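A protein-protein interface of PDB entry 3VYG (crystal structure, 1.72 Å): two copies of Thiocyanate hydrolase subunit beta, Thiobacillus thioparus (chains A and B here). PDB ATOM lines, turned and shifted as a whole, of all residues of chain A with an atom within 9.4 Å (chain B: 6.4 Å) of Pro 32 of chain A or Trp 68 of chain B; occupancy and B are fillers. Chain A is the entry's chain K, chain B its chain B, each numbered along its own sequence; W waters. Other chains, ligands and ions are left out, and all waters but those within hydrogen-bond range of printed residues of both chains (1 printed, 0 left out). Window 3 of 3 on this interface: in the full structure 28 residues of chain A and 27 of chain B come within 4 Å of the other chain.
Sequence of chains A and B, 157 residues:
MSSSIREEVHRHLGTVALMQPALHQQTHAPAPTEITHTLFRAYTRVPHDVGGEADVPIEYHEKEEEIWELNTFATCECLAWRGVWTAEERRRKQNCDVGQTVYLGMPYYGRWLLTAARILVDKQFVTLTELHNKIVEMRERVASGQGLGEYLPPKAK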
ATOM      1  N   ALA A  29       4.161  22.853  -4.796  1.00  0.00           N
ATOM      2  CA  ALA A  29       5.359  22.220  -5.307  1.00  0.00           C
ATOM      3  C   ALA A  29       5.143  20.795  -5.902  1.00  0.00           C
ATOM      4  O   ALA A  29       5.626  19.747  -5.348  1.00  0.00           O
ATOM      5  CB  ALA A  29       6.567  22.284  -4.215  1.00  0.00           C
ATOM      6  N   PRO A  30       4.323  20.730  -6.932  1.00  0.00           N
ATOM      7  CA  PRO A  30       3.964  19.470  -7.527  1.00  0.00           C
ATOM      8  C   PRO A  30       5.188  18.725  -8.040  1.00  0.00           C
ATOM      9  O   PRO A  30       6.197  19.347  -8.388  1.00  0.00           O
ATOM     10  CB  PRO A  30       3.057  19.859  -8.717  1.00  0.00           C
ATOM     11  CG  PRO A  30       2.666  21.226  -8.530  1.00  0.00           C
ATOM     12  CD  PRO A  30       3.669  21.860  -7.631  1.00  0.00           C
ATOM     13  N   ALA A  31       5.088  17.397  -8.105  1.00  0.00           N
ATOM     14  CA  ALA A  31       6.217  16.603  -8.656  1.00  0.00           C
ATOM     15  C   ALA A  31       6.318  16.850 -10.158  1.00  0.00           C
ATOM     16  O   ALA A  31       5.372  17.333 -10.831  1.00  0.00           O
ATOM     17  CB  ALA A  31       5.923  15.136  -8.421  1.00  0.00           C
ATOM     18  N   PRO A  32       7.480  16.593 -10.723  1.00  0.00           N
ATOM     19  CA  PRO A  32       7.648  16.811 -12.189  1.00  0.00           C
ATOM     20  C   PRO A  32       6.636  16.072 -13.102  1.00  0.00           C
ATOM     21  O   PRO A  32       6.227  16.528 -14.201  1.00  0.00           O
ATOM     22  CB  PRO A  32       9.077  16.310 -12.464  1.00  0.00           C
ATOM     23  CG  PRO A  32       9.734  16.312 -11.213  1.00  0.00           C
ATOM     24  CD  PRO A  32       8.738  16.158 -10.047  1.00  0.00           C
ATOM     25  N   THR A  33       6.121  14.953 -12.617  1.00  0.00           N
ATOM     26  CA  THR A  33       5.104  14.210 -13.392  1.00  0.00           C
ATOM     27  C   THR A  33       3.743  14.887 -13.462  1.00  0.00           C
ATOM     28  O   THR A  33       2.832  14.427 -14.167  1.00  0.00           O
ATOM     29  CB  THR A  33       4.933  12.819 -12.733  1.00  0.00           C
ATOM     30  OG1 THR A  33       4.915  12.965 -11.291  1.00  0.00           O
ATOM     31  CG2 THR A  33       6.172  11.957 -13.191  1.00  0.00           C
ATOM     32  N   GLU A  34       3.547  15.887 -12.646  1.00  0.00           N
ATOM     33  CA  GLU A  34       2.321  16.702 -12.664  1.00  0.00           C
ATOM     34  C   GLU A  34       2.413  17.920 -13.583  1.00  0.00           C
ATOM     35  O   GLU A  34       1.456  18.735 -13.601  1.00  0.00           O
ATOM     36  CB  GLU A  34       1.927  17.166 -11.224  1.00  0.00           C
ATOM     37  CG  GLU A  34       1.486  16.072 -10.247  1.00  0.00           C
ATOM     38  CD  GLU A  34       0.284  15.298 -10.763  1.00  0.00           C
ATOM     39  OE1 GLU A  34      -0.820  15.907 -10.958  1.00  0.00           O
ATOM     40  OE2 GLU A  34       0.451  14.075 -11.000  1.00  0.00           O
ATOM     41  N   ILE A  35       3.560  18.100 -14.255  1.00  0.00           N
ATOM     42  CA  ILE A  35       3.730  19.337 -15.071  1.00  0.00           C
ATOM     43  C   ILE A  35       3.764  18.896 -16.528  1.00  0.00           C
ATOM     44  O   ILE A  35       4.676  18.153 -16.965  1.00  0.00           O
ATOM     45  CB  ILE A  35       5.101  19.950 -14.755  1.00  0.00           C
ATOM     46  CG1 ILE A  35       5.173  20.394 -13.276  1.00  0.00           C
ATOM     47  CG2 ILE A  35       5.376  21.149 -15.721  1.00  0.00           C
ATOM     48  CD1 ILE A  35       4.166  21.385 -12.850  1.00  0.00           C
ATOM     49  N   THR A  36       2.689  19.205 -17.233  1.00  0.00           N
ATOM     50  CA  THR A  36       2.682  18.978 -18.711  1.00  0.00           C
ATOM     51  C   THR A  36       3.486  20.018 -19.421  1.00  0.00           C
ATOM     52  O   THR A  36       3.872  21.021 -18.808  1.00  0.00           O
ATOM     53  CB  THR A  36       1.212  19.153 -19.189  1.00  0.00           C
ATOM     54  OG1 THR A  36       0.716  20.428 -18.692  1.00  0.00           O
ATOM     55  CG2 THR A  36       0.296  18.111 -18.440  1.00  0.00           C
ATOM     56  N   HIS A  37       3.734  19.739 -20.720  1.00  0.00           N
ATOM     57  CA  HIS A  37       4.413  20.759 -21.538  1.00  0.00           C
ATOM     58  C   HIS A  37       3.578  22.081 -21.462  1.00  0.00           C
ATOM     59  O   HIS A  37       4.138  23.188 -21.351  1.00  0.00           O
ATOM     60  CB  HIS A  37       4.526  20.343 -22.992  1.00  0.00           C
ATOM     61  CG  HIS A  37       5.129  21.446 -23.863  1.00  0.00           C
ATOM     62  ND1 HIS A  37       4.389  22.213 -24.757  1.00  0.00           N
ATOM     63  CD2 HIS A  37       6.346  22.019 -23.786  1.00  0.00           C
ATOM     64  CE1 HIS A  37       5.175  23.162 -25.263  1.00  0.00           C
ATOM     65  NE2 HIS A  37       6.361  23.087 -24.670  1.00  0.00           N
ATOM     66  N   LEU A  39       1.632  23.261 -19.057  1.00  0.00           N
ATOM     67  CA  LEU A  39       1.990  23.950 -17.802  1.00  0.00           C
ATOM     68  C   LEU A  39       3.397  24.549 -17.717  1.00  0.00           C
ATOM     69  O   LEU A  39       3.589  25.619 -17.165  1.00  0.00           O
ATOM     70  CB  LEU A  39       1.665  23.035 -16.563  1.00  0.00           C
ATOM     71  CG  LEU A  39       0.159  22.935 -16.307  1.00  0.00           C
ATOM     72  CD1 LEU A  39       0.080  21.788 -15.212  1.00  0.00           C
ATOM     73  CD2 LEU A  39      -0.504  24.182 -15.853  1.00  0.00           C
ATOM     74  N   PHE A  40       4.366  23.833 -18.233  1.00  0.00           N
ATOM     75  CA  PHE A  40       5.726  24.277 -18.213  1.00  0.00           C
ATOM     76  C   PHE A  40       5.836  25.601 -19.013  1.00  0.00           C
ATOM     77  O   PHE A  40       6.482  26.505 -18.534  1.00  0.00           O
ATOM     78  CB  PHE A  40       6.652  23.168 -18.882  1.00  0.00           C
ATOM     79  CG  PHE A  40       8.139  23.558 -18.838  1.00  0.00           C
ATOM     80  CD1 PHE A  40       8.943  23.116 -17.807  1.00  0.00           C
ATOM     81  CD2 PHE A  40       8.686  24.394 -19.838  1.00  0.00           C
ATOM     82  CE1 PHE A  40      10.295  23.443 -17.717  1.00  0.00           C
ATOM     83  CE2 PHE A  40      10.040  24.811 -19.720  1.00  0.00           C
ATOM     84  CZ  PHE A  40      10.850  24.362 -18.725  1.00  0.00           C
ATOM     85  N   LYS B  63       9.639   9.992  -2.865  1.00  0.00           N
ATOM     86  CA  LYS B  63       9.573  10.118  -4.346  1.00  0.00           C
ATOM     87  C   LYS B  63      10.878   9.607  -4.893  1.00  0.00           C
ATOM     88  O   LYS B  63      11.948   9.925  -4.325  1.00  0.00           O
ATOM     89  CB  LYS B  63       9.314  11.533  -4.870  1.00  0.00           C
ATOM     90  CG  LYS B  63       9.134  11.522  -6.411  1.00  0.00           C
ATOM     91  CD  LYS B  63       8.904  12.991  -7.004  1.00  0.00           C
ATOM     92  CE  LYS B  63      10.292  13.697  -7.295  1.00  0.00           C
ATOM     93  NZ  LYS B  63      11.004  12.896  -8.397  1.00  0.00           N
ATOM     94  N   GLU B  65      14.048   9.498  -7.220  1.00  0.00           N
ATOM     95  CA  GLU B  65      14.816  10.538  -7.914  1.00  0.00           C
ATOM     96  C   GLU B  65      14.795  10.292  -9.432  1.00  0.00           C
ATOM     97  O   GLU B  65      15.100   9.204  -9.913  1.00  0.00           O
ATOM     98  CB  GLU B  65      16.213  10.476  -7.327  1.00  0.00           C
ATOM     99  CG  GLU B  65      17.290  11.488  -7.917  1.00  0.00           C
ATOM    100  CD  GLU B  65      18.720  11.309  -7.266  1.00  0.00           C
ATOM    101  OE1 GLU B  65      19.314  12.370  -6.960  1.00  0.00           O
ATOM    102  OE2 GLU B  65      19.321  10.163  -7.071  1.00  0.00           O
ATOM    103  N   GLU B  66      14.566  11.348 -10.199  1.00  0.00           N
ATOM    104  CA  GLU B  66      14.614  11.256 -11.686  1.00  0.00           C
ATOM    105  C   GLU B  66      16.063  11.370 -12.093  1.00  0.00           C
ATOM    106  O   GLU B  66      16.858  12.045 -11.450  1.00  0.00           O
ATOM    107  CB  GLU B  66      13.926  12.441 -12.339  1.00  0.00           C
ATOM    108  CG  GLU B  66      12.393  12.566 -12.192  1.00  0.00           C
ATOM    109  CD  GLU B  66      11.579  11.794 -13.252  1.00  0.00           C
ATOM    110  OE1 GLU B  66      12.200  11.178 -14.182  1.00  0.00           O
ATOM    111  OE2 GLU B  66      10.316  11.887 -13.071  1.00  0.00           O
ATOM    112  N   ILE B  67      16.425  10.697 -13.216  1.00  0.00           N
ATOM    113  CA  ILE B  67      17.782  10.933 -13.758  1.00  0.00           C
ATOM    114  C   ILE B  67      18.103  12.444 -13.929  1.00  0.00           C
ATOM    115  O   ILE B  67      19.222  12.862 -13.571  1.00  0.00           O
ATOM    116  CB  ILE B  67      17.970  10.198 -15.123  1.00  0.00           C
ATOM    117  CG1 ILE B  67      17.927   8.687 -14.869  1.00  0.00           C
ATOM    118  CG2 ILE B  67      19.201  10.624 -15.810  1.00  0.00           C
ATOM    119  CD1 ILE B  67      18.096   7.850 -16.116  1.00  0.00           C
ATOM    120  N   TRP B  68      17.124  13.220 -14.441  1.00  0.00           N
ATOM    121  CA  TRP B  68      17.383  14.643 -14.743  1.00  0.00           C
ATOM    122  C   TRP B  68      17.582  15.419 -13.404  1.00  0.00           C
ATOM    123  O   TRP B  68      18.300  16.404 -13.368  1.00  0.00           O
ATOM    124  CB  TRP B  68      16.269  15.293 -15.649  1.00  0.00           C
ATOM    125  CG  TRP B  68      14.917  15.561 -14.991  1.00  0.00           C
ATOM    126  CD1 TRP B  68      13.802  14.843 -15.100  1.00  0.00           C
ATOM    127  CD2 TRP B  68      14.590  16.729 -14.231  1.00  0.00           C
ATOM    128  NE1 TRP B  68      12.740  15.453 -14.406  1.00  0.00           N
ATOM    129  CE2 TRP B  68      13.241  16.609 -13.839  1.00  0.00           C
ATOM    130  CE3 TRP B  68      15.338  17.822 -13.823  1.00  0.00           C
ATOM    131  CZ2 TRP B  68      12.567  17.614 -13.054  1.00  0.00           C
ATOM    132  CZ3 TRP B  68      14.695  18.794 -12.984  1.00  0.00           C
ATOM    133  CH2 TRP B  68      13.327  18.681 -12.648  1.00  0.00           C
ATOM    134  N   GLU B  69      16.916  14.969 -12.312  1.00  0.00           N
ATOM    135  CA  GLU B  69      17.073  15.633 -10.992  1.00  0.00           C
ATOM    136  C   GLU B  69      18.444  15.407 -10.430  1.00  0.00           C
ATOM    137  O   GLU B  69      19.109  16.358 -10.014  1.00  0.00           O
ATOM    138  CB  GLU B  69      16.004  15.031 -10.031  1.00  0.00           C
ATOM    139  CG  GLU B  69      14.616  15.598 -10.358  1.00  0.00           C
ATOM    140  CD  GLU B  69      13.559  14.991  -9.450  1.00  0.00           C
ATOM    141  OE1 GLU B  69      13.831  13.851  -8.943  1.00  0.00           O
ATOM    142  OE2 GLU B  69      12.561  15.667  -9.181  1.00  0.00           O
ATOM    143  N   LEU B  70      18.973  14.164 -10.508  1.00  0.00           N
ATOM    144  CA  LEU B  70      20.338  13.881 -10.081  1.00  0.00           C
ATOM    145  C   LEU B  70      21.343  14.713 -10.940  1.00  0.00           C
ATOM    146  O   LEU B  70      22.292  15.283 -10.392  1.00  0.00           O
ATOM    147  CB  LEU B  70      20.652  12.373 -10.264  1.00  0.00           C
ATOM    148  CG  LEU B  70      22.103  12.006  -9.863  1.00  0.00           C
ATOM    149  CD1 LEU B  70      22.658  12.587  -8.474  1.00  0.00           C
ATOM    150  CD2 LEU B  70      22.254  10.510 -10.030  1.00  0.00           C
ATOM    151  N   ASN B  71      21.121  14.758 -12.267  1.00  0.00           N
ATOM    152  CA  ASN B  71      22.032  15.541 -13.132  1.00  0.00           C
ATOM    153  C   ASN B  71      21.970  17.031 -12.814  1.00  0.00           C
ATOM    154  O   ASN B  71      22.984  17.684 -12.762  1.00  0.00           O
ATOM    155  CB  ASN B  71      21.739  15.309 -14.624  1.00  0.00           C
ATOM    156  CG  ASN B  71      22.140  13.976 -15.131  1.00  0.00           C
ATOM    157  OD1 ASN B  71      21.458  13.405 -16.034  1.00  0.00           O
ATOM    158  ND2 ASN B  71      23.229  13.466 -14.665  1.00  0.00           N
ATOM    159  N   THR B  72      20.779  17.534 -12.481  1.00  0.00           N
ATOM    160  CA  THR B  72      20.608  18.984 -12.089  1.00  0.00           C
ATOM    161  C   THR B  72      21.367  19.262 -10.784  1.00  0.00           C
ATOM    162  O   THR B  72      22.052  20.273 -10.629  1.00  0.00           O
ATOM    163  CB  THR B  72      19.109  19.327 -11.971  1.00  0.00           C
ATOM    164  OG1 THR B  72      18.509  19.189 -13.266  1.00  0.00           O
ATOM    165  CG2 THR B  72      18.891  20.737 -11.430  1.00  0.00           C
ATOM    166  N   PHE B  73      21.158  18.396  -9.792  1.00  0.00           N
ATOM    167  CA  PHE B  73      21.798  18.576  -8.515  1.00  0.00           C
ATOM    168  C   PHE B  73      23.333  18.601  -8.690  1.00  0.00           C
ATOM    169  O   PHE B  73      24.023  19.463  -8.168  1.00  0.00           O
ATOM    170  CB  PHE B  73      21.343  17.392  -7.631  1.00  0.00           C
ATOM    171  CG  PHE B  73      21.855  17.421  -6.193  1.00  0.00           C
ATOM    172  CD1 PHE B  73      21.706  18.529  -5.390  1.00  0.00           C
ATOM    173  CD2 PHE B  73      22.206  16.224  -5.585  1.00  0.00           C
ATOM    174  CE1 PHE B  73      22.073  18.520  -4.034  1.00  0.00           C
ATOM    175  CE2 PHE B  73      22.555  16.166  -4.199  1.00  0.00           C
ATOM    176  CZ  PHE B  73      22.489  17.309  -3.423  1.00  0.00           C
ATOM    177  N   PRO B 107       8.007  22.247  -9.825  1.00  0.00           N
ATOM    178  CA  PRO B 107       8.670  21.276  -8.931  1.00  0.00           C
ATOM    179  C   PRO B 107       9.982  21.780  -8.346  1.00  0.00           C
ATOM    180  O   PRO B 107      10.636  22.621  -8.935  1.00  0.00           O
ATOM    181  CB  PRO B 107       8.932  20.039  -9.817  1.00  0.00           C
ATOM    182  CG  PRO B 107       8.127  20.319 -11.113  1.00  0.00           C
ATOM    183  CD  PRO B 107       8.157  21.819 -11.229  1.00  0.00           C
ATOM    184  N   TYR B 108      10.266  21.308  -7.131  1.00  0.00           N
ATOM    185  CA  TYR B 108      11.513  21.627  -6.388  1.00  0.00           C
ATOM    186  C   TYR B 108      12.729  21.539  -7.346  1.00  0.00           C
ATOM    187  O   TYR B 108      13.400  22.578  -7.513  1.00  0.00           O
ATOM    188  CB  TYR B 108      11.652  20.545  -5.335  1.00  0.00           C
ATOM    189  CG  TYR B 108      12.923  20.490  -4.546  1.00  0.00           C
ATOM    190  CD1 TYR B 108      13.045  21.227  -3.397  1.00  0.00           C
ATOM    191  CD2 TYR B 108      13.918  19.594  -4.884  1.00  0.00           C
ATOM    192  CE1 TYR B 108      14.193  21.126  -2.614  1.00  0.00           C
ATOM    193  CE2 TYR B 108      15.056  19.453  -4.107  1.00  0.00           C
ATOM    194  CZ  TYR B 108      15.151  20.261  -2.974  1.00  0.00           C
ATOM    195  OH  TYR B 108      16.291  20.179  -2.242  1.00  0.00           O
ATOM    196  N   TYR B 109      12.965  20.402  -8.034  1.00  0.00           N
ATOM    197  CA  TYR B 109      14.191  20.429  -8.855  1.00  0.00           C
ATOM    198  C   TYR B 109      13.988  21.127 -10.150  1.00  0.00           C
ATOM    199  O   TYR B 109      14.996  21.524 -10.761  1.00  0.00           O
ATOM    200  CB  TYR B 109      14.730  19.007  -9.116  1.00  0.00           C
ATOM    201  CG  TYR B 109      15.702  18.469  -8.081  1.00  0.00           C
ATOM    202  CD1 TYR B 109      15.402  17.322  -7.391  1.00  0.00           C
ATOM    203  CD2 TYR B 109      16.869  19.210  -7.705  1.00  0.00           C
ATOM    204  CE1 TYR B 109      16.297  16.833  -6.455  1.00  0.00           C
ATOM    205  CE2 TYR B 109      17.752  18.744  -6.843  1.00  0.00           C
ATOM    206  CZ  TYR B 109      17.463  17.566  -6.184  1.00  0.00           C
ATOM    207  OH  TYR B 109      18.353  17.030  -5.259  1.00  0.00           O
ATOM    208  N   GLY B 110      12.726  21.434 -10.514  1.00  0.00           N
ATOM    209  CA  GLY B 110      12.435  22.336 -11.650  1.00  0.00           C
ATOM    210  C   GLY B 110      13.104  23.684 -11.378  1.00  0.00           C
ATOM    211  O   GLY B 110      13.657  24.309 -12.288  1.00  0.00           O
ATOM    212  N   ARG B 111      12.925  24.167 -10.122  1.00  0.00           N
ATOM    213  CA  ARG B 111      13.496  25.487  -9.725  1.00  0.00           C
ATOM    214  C   ARG B 111      15.032  25.443  -9.705  1.00  0.00           C
ATOM    215  O   ARG B 111      15.702  26.419 -10.141  1.00  0.00           O
ATOM    216  CB  ARG B 111      12.934  26.025  -8.396  1.00  0.00           C
ATOM    217  CG  ARG B 111      11.434  26.251  -8.529  1.00  0.00           C
ATOM    218  CD  ARG B 111      10.745  26.773  -7.265  1.00  0.00           C
ATOM    219  NE  ARG B 111      10.933  25.837  -6.142  1.00  0.00           N
ATOM    220  CZ  ARG B 111      11.875  25.921  -5.209  1.00  0.00           C
ATOM    221  NH1 ARG B 111      12.816  26.894  -5.263  1.00  0.00           N
ATOM    222  NH2 ARG B 111      11.877  25.034  -4.221  1.00  0.00           N
ATOM    223  N   LEU B 113      16.784  23.637 -11.574  1.00  0.00           N
ATOM    224  CA  LEU B 113      17.296  23.587 -13.000  1.00  0.00           C
ATOM    225  C   LEU B 113      17.125  24.916 -13.673  1.00  0.00           C
ATOM    226  O   LEU B 113      18.028  25.400 -14.378  1.00  0.00           O
ATOM    227  CB  LEU B 113      16.587  22.479 -13.779  1.00  0.00           C
ATOM    228  CG  LEU B 113      16.906  22.445 -15.298  1.00  0.00           C
ATOM    229  CD1 LEU B 113      18.395  22.229 -15.570  1.00  0.00           C
ATOM    230  CD2 LEU B 113      16.153  21.166 -15.872  1.00  0.00           C
ATOM    231  N   TYR B 151      18.642   9.817 -21.676  1.00  0.00           N
ATOM    232  CA  TYR B 151      17.169  10.002 -21.650  1.00  0.00           C
ATOM    233  C   TYR B 151      16.494   9.263 -22.794  1.00  0.00           C
ATOM    234  O   TYR B 151      15.339   8.842 -22.677  1.00  0.00           O
ATOM    235  CB  TYR B 151      16.760  11.483 -21.738  1.00  0.00           C
ATOM    236  CG  TYR B 151      17.340  12.280 -20.609  1.00  0.00           C
ATOM    237  CD1 TYR B 151      18.234  13.319 -20.866  1.00  0.00           C
ATOM    238  CD2 TYR B 151      17.015  12.008 -19.294  1.00  0.00           C
ATOM    239  CE1 TYR B 151      18.789  14.047 -19.846  1.00  0.00           C
ATOM    240  CE2 TYR B 151      17.595  12.738 -18.231  1.00  0.00           C
ATOM    241  CZ  TYR B 151      18.470  13.744 -18.531  1.00  0.00           C
ATOM    242  OH  TYR B 151      19.032  14.449 -17.527  1.00  0.00           O
HETATM  243  O   HOH W   1       8.353  19.466  -5.847  1.00  0.00           O
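No position is printed for both chains.
Of the 6 pairs that touch across the chains among the printed residues, none has its exchanged pair printed and touching as well.
NZ of Lys 63 of chain B is in salt-bridge range of OE1 of Glu 69 of chain B (3.0 Å).
N of Glu 66 of chain B lies within hydrogen-bond range of OE1 of Glu 69 of chain B.
O of Trp 68 of chain B lies within hydrogen-bond range of OG1 of Thr 72 of chain B, at 2.8 Å.
Of the printed residues of chain B, Pro 32 of chain A touches Trp 68, Glu 69 and Pro 107.
Of chain A, only Pro 32 comes within 4 Å of Trp 68 of chain B.
No residue of chain A comes within 4 Å of Glu 66 of chain B.
Of chain A, only Pro 32 comes within 4 Å of Glu 69 of chain B.
Of the printed residues of chain A, Lys 63 of chain B touches Ala 31 (3.9 Å).
Printed residues of chain B within 4 Å of Pro 30 of chain A: Pro 107 (3.2 Å).
Of the printed residues of chain B, Ala 31 of chain A touches Lys 63.
Thr 36 of chain A touches none of the printed residues of chain B.
The nearest printed residue of chain A that does not touch Lys 63 of chain B is Pro 32 of chain A (4.01 Å).
Among the printed residues, merely in contact across the chains: Pro 30 of chain A with Pro 107 of chain B, Ala 31 of chain A with Lys 63 of chain B, Pro 32 of chain A with Trp 68 of chain B, Pro 32 of chain A with Glu 69 of chain B, Pro 32 of chain A with Pro 107 of chain B and Ile 35 of chain A with Pro 107 of chain B.
Water W1 lies within hydrogen-bond range of O of Ala 29 of chain A (2.8 Å), N of Tyr 108 of chain B (2.9 Å) and O of Pro 30 of chain A (3.3 Å).
Of the 11 printed residues of chain A, 4 touch a printed residue of chain B.
Hydrophobic or aromatic side chains of chain A within 4 Å of the printed part of chain B: Ala 31, Pro 32 and Ile 35.
Hydrophobic or aromatic side chains of chain B within 4 Å of the printed part of chain A: Trp 68 and Pro 107.
Among the printed residues, no Asp or Glu carboxylate lies within 4 Å of a Lys or Arg side-chain nitrogen of the other chain.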
